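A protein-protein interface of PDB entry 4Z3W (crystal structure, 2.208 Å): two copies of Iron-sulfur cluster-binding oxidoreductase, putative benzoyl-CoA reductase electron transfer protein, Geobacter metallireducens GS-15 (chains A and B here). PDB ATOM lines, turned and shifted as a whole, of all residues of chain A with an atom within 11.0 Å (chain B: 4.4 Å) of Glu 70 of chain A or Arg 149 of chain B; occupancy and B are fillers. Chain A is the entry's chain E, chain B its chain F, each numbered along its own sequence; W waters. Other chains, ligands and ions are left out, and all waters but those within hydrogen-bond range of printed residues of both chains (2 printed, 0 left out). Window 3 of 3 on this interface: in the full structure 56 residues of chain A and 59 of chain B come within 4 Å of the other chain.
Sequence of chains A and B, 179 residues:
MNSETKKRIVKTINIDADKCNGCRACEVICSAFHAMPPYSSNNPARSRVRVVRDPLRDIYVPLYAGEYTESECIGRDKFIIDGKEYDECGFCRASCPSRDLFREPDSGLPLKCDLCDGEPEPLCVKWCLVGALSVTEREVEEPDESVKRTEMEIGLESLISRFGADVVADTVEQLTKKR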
ATOM      1  N   GLY A  66       4.216 -11.253 -27.893  1.00  0.00           N
ATOM      2  CA  GLY A  66       5.446 -11.870 -27.434  1.00  0.00           C
ATOM      3  C   GLY A  66       5.661 -11.739 -25.943  1.00  0.00           C
ATOM      4  O   GLY A  66       4.845 -12.189 -25.138  1.00  0.00           O
ATOM      5  N   GLU A  67       6.747 -11.069 -25.576  1.00  0.00           N
ATOM      6  CA  GLU A  67       7.232 -10.988 -24.202  1.00  0.00           C
ATOM      7  C   GLU A  67       6.505  -9.927 -23.384  1.00  0.00           C
ATOM      8  O   GLU A  67       6.188  -8.860 -23.906  1.00  0.00           O
ATOM      9  CB  GLU A  67       8.744 -10.692 -24.200  1.00  0.00           C
ATOM     10  CG  GLU A  67       9.152  -9.324 -24.801  1.00  0.00           C
ATOM     11  CD  GLU A  67       9.002  -9.253 -26.324  1.00  0.00           C
ATOM     12  OE1 GLU A  67       8.440 -10.186 -26.930  1.00  0.00           O
ATOM     13  OE2 GLU A  67       9.448  -8.255 -26.925  1.00  0.00           O
ATOM     14  N   TYR A  68       6.275 -10.212 -22.106  1.00  0.00           N
ATOM     15  CA  TYR A  68       5.766  -9.216 -21.187  1.00  0.00           C
ATOM     16  C   TYR A  68       6.930  -8.356 -20.700  1.00  0.00           C
ATOM     17  O   TYR A  68       8.038  -8.859 -20.508  1.00  0.00           O
ATOM     18  CB  TYR A  68       5.051  -9.871 -20.002  1.00  0.00           C
ATOM     19  CG  TYR A  68       4.750  -8.906 -18.869  1.00  0.00           C
ATOM     20  CD1 TYR A  68       3.640  -8.051 -18.920  1.00  0.00           C
ATOM     21  CD2 TYR A  68       5.575  -8.840 -17.752  1.00  0.00           C
ATOM     22  CE1 TYR A  68       3.362  -7.161 -17.885  1.00  0.00           C
ATOM     23  CE2 TYR A  68       5.306  -7.951 -16.711  1.00  0.00           C
ATOM     24  CZ  TYR A  68       4.202  -7.119 -16.787  1.00  0.00           C
ATOM     25  OH  TYR A  68       3.947  -6.254 -15.753  1.00  0.00           O
ATOM     26  N   THR A  69       6.684  -7.062 -20.533  1.00  0.00           N
ATOM     27  CA  THR A  69       7.661  -6.162 -19.943  1.00  0.00           C
ATOM     28  C   THR A  69       6.949  -5.230 -18.973  1.00  0.00           C
ATOM     29  O   THR A  69       5.853  -4.742 -19.252  1.00  0.00           O
ATOM     30  CB  THR A  69       8.402  -5.334 -21.004  1.00  0.00           C
ATOM     31  OG1 THR A  69       9.186  -4.326 -20.351  1.00  0.00           O
ATOM     32  CG2 THR A  69       7.419  -4.645 -21.913  1.00  0.00           C
ATOM     33  N   GLU A  70       7.573  -4.981 -17.832  1.00  0.00           N
ATOM     34  CA  GLU A  70       6.930  -4.203 -16.792  1.00  0.00           C
ATOM     35  C   GLU A  70       7.165  -2.717 -17.022  1.00  0.00           C
ATOM     36  O   GLU A  70       6.613  -1.869 -16.307  1.00  0.00           O
ATOM     37  CB  GLU A  70       7.446  -4.616 -15.415  1.00  0.00           C
ATOM     38  CG  GLU A  70       8.867  -4.120 -15.131  1.00  0.00           C
ATOM     39  CD  GLU A  70       9.504  -4.770 -13.902  1.00  0.00           C
ATOM     40  OE1 GLU A  70       8.755  -5.239 -13.011  1.00  0.00           O
ATOM     41  OE2 GLU A  70      10.756  -4.825 -13.844  1.00  0.00           O
ATOM     42  N   SER A  71       7.976  -2.391 -18.027  1.00  0.00           N
ATOM     43  CA  SER A  71       8.302  -0.988 -18.260  1.00  0.00           C
ATOM     44  C   SER A  71       8.653  -0.696 -19.698  1.00  0.00           C
ATOM     45  O   SER A  71       9.088  -1.585 -20.434  1.00  0.00           O
ATOM     46  CB  SER A  71       9.463  -0.554 -17.361  1.00  0.00           C
ATOM     47  OG  SER A  71      10.672  -1.121 -17.813  1.00  0.00           O
ATOM     48  N   GLU A  72       8.444   0.560 -20.085  1.00  0.00           N
ATOM     49  CA  GLU A  72       8.777   1.056 -21.417  1.00  0.00           C
ATOM     50  C   GLU A  72      10.271   1.124 -21.629  1.00  0.00           C
ATOM     51  O   GLU A  72      11.045   1.076 -20.678  1.00  0.00           O
ATOM     52  CB  GLU A  72       8.199   2.457 -21.643  1.00  0.00           C
ATOM     53  CG  GLU A  72       6.676   2.545 -21.740  1.00  0.00           C
ATOM     54  CD  GLU A  72       6.201   3.988 -21.831  1.00  0.00           C
ATOM     55  OE1 GLU A  72       5.057   4.262 -21.403  1.00  0.00           O
ATOM     56  OE2 GLU A  72       6.981   4.849 -22.312  1.00  0.00           O
ATOM     57  N   CYS A  73      10.666   1.271 -22.888  1.00  0.00           N
ATOM     58  CA  CYS A  73      12.051   1.558 -23.214  1.00  0.00           C
ATOM     59  C   CYS A  73      12.347   3.034 -22.999  1.00  0.00           C
ATOM     60  O   CYS A  73      11.458   3.882 -23.115  1.00  0.00           O
ATOM     61  CB  CYS A  73      12.353   1.175 -24.663  1.00  0.00           C
ATOM     62  SG  CYS A  73      12.269  -0.589 -24.970  1.00  0.00           S
ATOM     63  N   ILE A  74      13.606   3.331 -22.723  1.00  0.00           N
ATOM     64  CA  ILE A  74      14.063   4.701 -22.547  1.00  0.00           C
ATOM     65  C   ILE A  74      13.853   5.511 -23.833  1.00  0.00           C
ATOM     66  O   ILE A  74      13.386   6.649 -23.796  1.00  0.00           O
ATOM     67  CB  ILE A  74      15.546   4.715 -22.110  1.00  0.00           C
ATOM     68  CG1 ILE A  74      15.632   4.338 -20.632  1.00  0.00           C
ATOM     69  CG2 ILE A  74      16.167   6.073 -22.324  1.00  0.00           C
ATOM     70  CD1 ILE A  74      17.024   4.074 -20.153  1.00  0.00           C
ATOM     71  N   CYS A  92       7.453  -4.362 -32.488  1.00  0.00           N
ATOM     72  CA  CYS A  92       7.622  -4.911 -31.164  1.00  0.00           C
ATOM     73  C   CYS A  92       6.485  -5.837 -30.748  1.00  0.00           C
ATOM     74  O   CYS A  92       5.323  -5.480 -30.833  1.00  0.00           O
ATOM     75  CB  CYS A  92       7.760  -3.781 -30.155  1.00  0.00           C
ATOM     76  SG  CYS A  92       8.127  -4.399 -28.540  1.00  0.00           S
ATOM     77  N   ALA A  94       5.951  -6.873 -27.680  1.00  0.00           N
ATOM     78  CA  ALA A  94       5.832  -6.854 -26.225  1.00  0.00           C
ATOM     79  C   ALA A  94       4.447  -6.462 -25.728  1.00  0.00           C
ATOM     80  O   ALA A  94       3.775  -5.592 -26.305  1.00  0.00           O
ATOM     81  CB  ALA A  94       6.871  -5.915 -25.621  1.00  0.00           C
ATOM     82  N   SER A  95       4.038  -7.111 -24.641  1.00  0.00           N
ATOM     83  CA  SER A  95       2.955  -6.602 -23.816  1.00  0.00           C
ATOM     84  C   SER A  95       3.559  -5.548 -22.893  1.00  0.00           C
ATOM     85  O   SER A  95       4.095  -5.868 -21.833  1.00  0.00           O
ATOM     86  CB  SER A  95       2.291  -7.724 -23.020  1.00  0.00           C
ATOM     87  OG  SER A  95       0.944  -7.406 -22.742  1.00  0.00           O
ATOM     88  N   CYS A  96       3.483  -4.291 -23.322  1.00  0.00           N
ATOM     89  CA  CYS A  96       4.246  -3.198 -22.730  1.00  0.00           C
ATOM     90  C   CYS A  96       3.320  -2.075 -22.257  1.00  0.00           C
ATOM     91  O   CYS A  96       2.215  -1.922 -22.776  1.00  0.00           O
ATOM     92  CB  CYS A  96       5.268  -2.697 -23.760  1.00  0.00           C
ATOM     93  SG  CYS A  96       5.916  -1.063 -23.521  1.00  0.00           S
ATOM     94  N   PRO A  97       3.745  -1.292 -21.261  1.00  0.00           N
ATOM     95  CA  PRO A  97       2.757  -0.330 -20.754  1.00  0.00           C
ATOM     96  C   PRO A  97       2.534   0.901 -21.647  1.00  0.00           C
ATOM     97  O   PRO A  97       1.639   1.695 -21.361  1.00  0.00           O
ATOM     98  CB  PRO A  97       3.324   0.083 -19.389  1.00  0.00           C
ATOM     99  CG  PRO A  97       4.807  -0.215 -19.446  1.00  0.00           C
ATOM    100  CD  PRO A  97       4.954  -1.381 -20.409  1.00  0.00           C
ATOM    101  N   SER A  98       3.306   1.032 -22.722  1.00  0.00           N
ATOM    102  CA  SER A  98       3.189   2.168 -23.648  1.00  0.00           C
ATOM    103  C   SER A  98       1.968   2.119 -24.584  1.00  0.00           C
ATOM    104  O   SER A  98       1.629   3.111 -25.213  1.00  0.00           O
ATOM    105  CB  SER A  98       4.446   2.257 -24.517  1.00  0.00           C
ATOM    106  OG  SER A  98       4.453   1.212 -25.482  1.00  0.00           O
ATOM    107  N   ARG A  99       1.328   0.965 -24.711  1.00  0.00           N
ATOM    108  CA  ARG A  99       0.212   0.867 -25.631  1.00  0.00           C
ATOM    109  C   ARG A  99      -0.717  -0.280 -25.282  1.00  0.00           C
ATOM    110  O   ARG A  99      -0.431  -1.074 -24.386  1.00  0.00           O
ATOM    111  CB  ARG A  99       0.712   0.711 -27.070  1.00  0.00           C
ATOM    112  CG  ARG A  99       1.151  -0.699 -27.450  1.00  0.00           C
ATOM    113  CD  ARG A  99       2.534  -1.018 -26.929  1.00  0.00           C
ATOM    114  NE  ARG A  99       2.951  -2.365 -27.309  1.00  0.00           N
ATOM    115  CZ  ARG A  99       3.379  -2.695 -28.522  1.00  0.00           C
ATOM    116  NH1 ARG A  99       3.450  -1.770 -29.471  1.00  0.00           N
ATOM    117  NH2 ARG A  99       3.745  -3.943 -28.789  1.00  0.00           N
ATOM    118  N   ARG A 103      -2.877  -6.656 -24.791  1.00  0.00           N
ATOM    119  CA  ARG A 103      -3.374  -6.483 -23.431  1.00  0.00           C
ATOM    120  C   ARG A 103      -4.892  -6.504 -23.432  1.00  0.00           C
ATOM    121  O   ARG A 103      -5.517  -5.850 -24.269  1.00  0.00           O
ATOM    122  CB  ARG A 103      -2.874  -5.171 -22.846  1.00  0.00           C
ATOM    123  CG  ARG A 103      -1.361  -5.043 -22.831  1.00  0.00           C
ATOM    124  CD  ARG A 103      -0.967  -3.694 -22.322  1.00  0.00           C
ATOM    125  NE  ARG A 103      -1.451  -3.487 -20.964  1.00  0.00           N
ATOM    126  CZ  ARG A 103      -1.308  -2.348 -20.297  1.00  0.00           C
ATOM    127  NH1 ARG A 103      -0.708  -1.319 -20.884  1.00  0.00           N
ATOM    128  NH2 ARG A 103      -1.772  -2.232 -19.052  1.00  0.00           N
ATOM    129  N   GLY A 108      -6.361  -5.006 -18.888  1.00  0.00           N
ATOM    130  CA  GLY A 108      -5.041  -4.521 -19.252  1.00  0.00           C
ATOM    131  C   GLY A 108      -3.991  -5.589 -19.016  1.00  0.00           C
ATOM    132  O   GLY A 108      -2.797  -5.354 -19.215  1.00  0.00           O
ATOM    133  N   PRO A 110      -1.720  -8.877 -19.694  1.00  0.00           N
ATOM    134  CA  PRO A 110      -0.941  -9.231 -20.886  1.00  0.00           C
ATOM    135  C   PRO A 110      -1.483 -10.456 -21.624  1.00  0.00           C
ATOM    136  O   PRO A 110      -1.990 -11.379 -20.993  1.00  0.00           O
ATOM    137  CB  PRO A 110       0.456  -9.510 -20.322  1.00  0.00           C
ATOM    138  CG  PRO A 110       0.229  -9.900 -18.911  1.00  0.00           C
ATOM    139  CD  PRO A 110      -0.972  -9.127 -18.448  1.00  0.00           C
ATOM    140  N   PHE A 163      29.238  -0.862 -10.552  1.00  0.00           N
ATOM    141  CA  PHE A 163      28.432  -0.231  -9.501  1.00  0.00           C
ATOM    142  C   PHE A 163      29.047  -0.283  -8.108  1.00  0.00           C
ATOM    143  O   PHE A 163      28.507   0.303  -7.169  1.00  0.00           O
ATOM    144  CB  PHE A 163      27.044  -0.867  -9.445  1.00  0.00           C
ATOM    145  CG  PHE A 163      26.283  -0.753 -10.723  1.00  0.00           C
ATOM    146  CD1 PHE A 163      25.839   0.480 -11.168  1.00  0.00           C
ATOM    147  CD2 PHE A 163      26.012  -1.874 -11.481  1.00  0.00           C
ATOM    148  CE1 PHE A 163      25.130   0.596 -12.353  1.00  0.00           C
ATOM    149  CE2 PHE A 163      25.301  -1.768 -12.672  1.00  0.00           C
ATOM    150  CZ  PHE A 163      24.858  -0.526 -13.105  1.00  0.00           C
ATOM    151  N   THR A 171      22.498  -4.939  -2.195  1.00  0.00           N
ATOM    152  CA  THR A 171      21.363  -5.260  -3.060  1.00  0.00           C
ATOM    153  C   THR A 171      21.012  -6.742  -3.027  1.00  0.00           C
ATOM    154  O   THR A 171      19.859  -7.107  -2.805  1.00  0.00           O
ATOM    155  CB  THR A 171      21.634  -4.855  -4.514  1.00  0.00           C
ATOM    156  OG1 THR A 171      21.801  -3.435  -4.590  1.00  0.00           O
ATOM    157  CG2 THR A 171      20.468  -5.276  -5.425  1.00  0.00           C
ATOM    158  N   GLN A 174      18.364  -8.914  -0.694  1.00  0.00           N
ATOM    159  CA  GLN A 174      17.009  -8.444  -0.983  1.00  0.00           C
ATOM    160  C   GLN A 174      16.476  -9.198  -2.193  1.00  0.00           C
ATOM    161  O   GLN A 174      17.231  -9.868  -2.897  1.00  0.00           O
ATOM    162  CB  GLN A 174      16.974  -6.934  -1.243  1.00  0.00           C
ATOM    163  N   GLU B 145       3.530   4.303 -16.729  1.00  0.00           N
ATOM    164  CA  GLU B 145       3.179   3.199 -15.830  1.00  0.00           C
ATOM    165  C   GLU B 145       4.320   2.214 -15.638  1.00  0.00           C
ATOM    166  O   GLU B 145       4.112   1.121 -15.115  1.00  0.00           O
ATOM    167  CB  GLU B 145       1.963   2.430 -16.351  1.00  0.00           C
ATOM    168  CG  GLU B 145       0.688   2.710 -15.600  1.00  0.00           C
ATOM    169  CD  GLU B 145       0.188   4.111 -15.856  1.00  0.00           C
ATOM    170  OE1 GLU B 145       0.667   4.733 -16.833  1.00  0.00           O
ATOM    171  OE2 GLU B 145      -0.672   4.587 -15.081  1.00  0.00           O
ATOM    172  N   SER B 146       5.513   2.582 -16.087  1.00  0.00           N
ATOM    173  CA  SER B 146       6.643   1.670 -16.003  1.00  0.00           C
ATOM    174  C   SER B 146       7.034   1.438 -14.555  1.00  0.00           C
ATOM    175  O   SER B 146       7.087   2.373 -13.760  1.00  0.00           O
ATOM    176  CB  SER B 146       7.838   2.208 -16.787  1.00  0.00           C
ATOM    177  OG  SER B 146       7.506   2.380 -18.152  1.00  0.00           O
ATOM    178  N   VAL B 147       7.263   0.179 -14.210  1.00  0.00           N
ATOM    179  CA  VAL B 147       7.975  -0.149 -12.986  1.00  0.00           C
ATOM    180  C   VAL B 147       9.444   0.071 -13.285  1.00  0.00           C
ATOM    181  O   VAL B 147      10.058  -0.727 -13.993  1.00  0.00           O
ATOM    182  CB  VAL B 147       7.732  -1.596 -12.532  1.00  0.00           C
ATOM    183  CG1 VAL B 147       8.623  -1.935 -11.338  1.00  0.00           C
ATOM    184  CG2 VAL B 147       6.261  -1.809 -12.196  1.00  0.00           C
ATOM    185  N   LYS B 148      10.003   1.163 -12.779  1.00  0.00           N
ATOM    186  CA  LYS B 148      11.358   1.544 -13.158  1.00  0.00           C
ATOM    187  C   LYS B 148      12.406   0.838 -12.299  1.00  0.00           C
ATOM    188  O   LYS B 148      12.639   1.217 -11.152  1.00  0.00           O
ATOM    189  CB  LYS B 148      11.532   3.062 -13.067  1.00  0.00           C
ATOM    190  CG  LYS B 148      10.618   3.860 -13.985  1.00  0.00           C
ATOM    191  CD  LYS B 148      11.390   4.966 -14.686  1.00  0.00           C
ATOM    192  CE  LYS B 148      12.231   5.760 -13.695  1.00  0.00           C
ATOM    193  NZ  LYS B 148      13.360   6.498 -14.342  1.00  0.00           N
ATOM    194  N   ARG B 149      13.027  -0.193 -12.861  1.00  0.00           N
ATOM    195  CA  ARG B 149      14.074  -0.934 -12.167  1.00  0.00           C
ATOM    196  C   ARG B 149      15.452  -0.525 -12.654  1.00  0.00           C
ATOM    197  O   ARG B 149      15.649  -0.308 -13.850  1.00  0.00           O
ATOM    198  CB  ARG B 149      13.898  -2.441 -12.358  1.00  0.00           C
ATOM    199  CG  ARG B 149      13.058  -3.106 -11.296  1.00  0.00           C
ATOM    200  CD  ARG B 149      12.991  -4.605 -11.524  1.00  0.00           C
ATOM    201  NE  ARG B 149      11.637  -5.101 -11.307  1.00  0.00           N
ATOM    202  CZ  ARG B 149      11.056  -5.192 -10.114  1.00  0.00           C
ATOM    203  NH1 ARG B 149      11.718  -4.821  -9.017  1.00  0.00           N
ATOM    204  NH2 ARG B 149       9.809  -5.647 -10.017  1.00  0.00           N
ATOM    205  N   THR B 150      16.407  -0.435 -11.727  1.00  0.00           N
ATOM    206  CA  THR B 150      17.773  -0.081 -12.091  1.00  0.00           C
ATOM    207  C   THR B 150      18.452  -1.195 -12.899  1.00  0.00           C
ATOM    208  O   THR B 150      18.192  -2.385 -12.684  1.00  0.00           O
ATOM    209  CB  THR B 150      18.636   0.226 -10.847  1.00  0.00           C
ATOM    210  OG1 THR B 150      18.557  -0.863  -9.918  1.00  0.00           O
ATOM    211  CG2 THR B 150      18.164   1.497 -10.171  1.00  0.00           C
ATOM    212  N   GLU B 151      19.297  -0.789 -13.844  1.00  0.00           N
ATOM    213  CA  GLU B 151      20.245  -1.687 -14.511  1.00  0.00           C
ATOM    214  C   GLU B 151      20.873  -2.660 -13.519  1.00  0.00           C
ATOM    215  O   GLU B 151      20.979  -3.868 -13.756  1.00  0.00           O
ATOM    216  CB  GLU B 151      21.343  -0.868 -15.196  1.00  0.00           C
ATOM    217  CG  GLU B 151      22.536  -1.658 -15.706  1.00  0.00           C
ATOM    218  CD  GLU B 151      23.498  -0.781 -16.503  1.00  0.00           C
ATOM    219  OE1 GLU B 151      23.337   0.457 -16.459  1.00  0.00           O
ATOM    220  OE2 GLU B 151      24.403  -1.321 -17.180  1.00  0.00           O
ATOM    221  N   GLU B 153      19.710  -3.582 -10.573  1.00  0.00           N
ATOM    222  CA  GLU B 153      18.726  -4.503 -10.044  1.00  0.00           C
ATOM    223  C   GLU B 153      18.357  -5.550 -11.105  1.00  0.00           C
ATOM    224  O   GLU B 153      18.252  -6.741 -10.798  1.00  0.00           O
ATOM    225  CB  GLU B 153      17.493  -3.739  -9.570  1.00  0.00           C
ATOM    226  CG  GLU B 153      16.748  -4.393  -8.422  1.00  0.00           C
ATOM    227  CD  GLU B 153      15.489  -3.622  -8.048  1.00  0.00           C
ATOM    228  OE1 GLU B 153      15.492  -2.375  -8.207  1.00  0.00           O
ATOM    229  OE2 GLU B 153      14.498  -4.263  -7.618  1.00  0.00           O
ATOM    230  N   ILE B 154      18.181  -5.111 -12.353  1.00  0.00           N
ATOM    231  CA  ILE B 154      17.862  -6.036 -13.445  1.00  0.00           C
ATOM    232  C   ILE B 154      19.013  -7.034 -13.648  1.00  0.00           C
ATOM    233  O   ILE B 154      18.793  -8.248 -13.753  1.00  0.00           O
ATOM    234  CB  ILE B 154      17.559  -5.283 -14.761  1.00  0.00           C
ATOM    235  CG1 ILE B 154      16.299  -4.431 -14.602  1.00  0.00           C
ATOM    236  CG2 ILE B 154      17.333  -6.259 -15.924  1.00  0.00           C
ATOM    237  CD1 ILE B 154      16.123  -3.411 -15.697  1.00  0.00           C
ATOM    238  N   GLU B 157      18.973  -9.643 -10.733  1.00  0.00           N
ATOM    239  CA  GLU B 157      17.811 -10.519 -10.838  1.00  0.00           C
ATOM    240  C   GLU B 157      17.963 -11.520 -11.989  1.00  0.00           C
ATOM    241  O   GLU B 157      17.491 -12.653 -11.882  1.00  0.00           O
ATOM    242  CB  GLU B 157      16.525  -9.703 -11.011  1.00  0.00           C
ATOM    243  CG  GLU B 157      15.831  -9.339  -9.699  1.00  0.00           C
ATOM    244  CD  GLU B 157      14.805  -8.210  -9.857  1.00  0.00           C
ATOM    245  OE1 GLU B 157      13.862  -8.357 -10.677  1.00  0.00           O
ATOM    246  OE2 GLU B 157      14.945  -7.172  -9.167  1.00  0.00           O
HETATM  247  O   HOH W   1       4.282  -1.793 -15.335  1.00  0.00           O
HETATM  248  O   HOH W   2       3.304   3.905 -19.681  1.00  0.00           O
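The backbone carbonyl oxygen (O) of Glu 70 of chain A lies within hydrogen-bond range of the backbone NH (N) of Val 147 of chain B (3.0 Å). The backbone NH (N) of Glu 72 of chain A sits at hydrogen-bond distance from the side-chain hydroxyl (OG) of Ser 146 of chain B (2.8 Å). The side-chain carboxylate (OE2) of Glu 70 of chain A is in salt-bridge range of the guanidinium group (NE) of Arg 149 of chain B, 2.7 Å away.
No position is printed for both chains.
Water W2 lies within hydrogen-bond range of OE1 of Glu 72 of chain A (2.5 Å), N of Glu 145 of chain B (3.0 Å) and O of Pro 97 of chain A (3.2 Å). Water W1 bridges the backbone carbonyl oxygen of Glu 70 of chain A (2.5 Å) and the backbone carbonyl oxygen of Glu 145 of chain B (2.9 Å).
Glu 70 of chain A touches just these residues of chain B: Ser 146 (3.6 Å), Val 147 (3.0 Å) and Arg 149 (2.7 Å). Printed residues of chain B within 4 Å of Ser 71 of chain A: Ser 146 and Val 147. Of the printed residues of chain B, Pro 97 of chain A touches Ser 146 (3.96 Å). Ser 146 of chain B touches just these residues of chain A: Glu 70, Ser 71, Glu 72 and Pro 97. Printed residues of chain A within 4 Å of Val 147 of chain B: Glu 70 (3.0 Å) and Ser 71 (3.4 Å). No residue of chain A comes within 4 Å of Lys 148 of chain B. Arg 149 of chain B touches just one residue of chain A: Glu 70. Printed residues of chain A within 4 Å of Glu 151 of chain B: Phe 163 (3.7 Å). No residue of chain A comes within 4 Å of Glu 153 of chain B. The nearest residue of chain B that does not touch Glu 70 of chain A is Glu 145 of chain B (4.1 Å). The nearest residue of chain A that does not touch Arg 149 of chain B is Ser 71 of chain A (5.6 Å).
Of the 22 printed residues of chain A, 5 touch a printed residue of chain B. Hydrophobic or aromatic side chains of chain A that line the printed part of chain B: Pro 97 and Phe 163. Printed residues of chain B that touch a printed residue of chain A: Ser 146, Val 147, Arg 149 and Glu 151. Among the printed residues, 8 pairs touch across the chains.
NE of Arg 149 of chain B lies within salt-bridge range of OE1 of Glu 157 of chain B, at 3.99 Å. The guanidinium group (NH1) of Arg 149 of chain B is in salt-bridge range of the side-chain carboxylate (OE2) of Glu 153 of chain B. OG1 of Thr 69 of chain A is in hydrogen-bond range of O of Ser 71 of chain A.
Ser 146 of chain B touches Glu 70 of chain A (CA to O, 3.6 Å). Ser 71 of chain A touches Ser 146 of chain B (CB to CB, 3.3 Å). CB of Ser 71 of chain A touches O of Val 147 of chain B, at 3.4 Å. Ser 146 of chain B touches Pro 97 of chain A (OG to CG, 3.96 Å). Phe 163 of chain A touches Glu 151 of chain B (CZ to CG, 3.7 Å).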
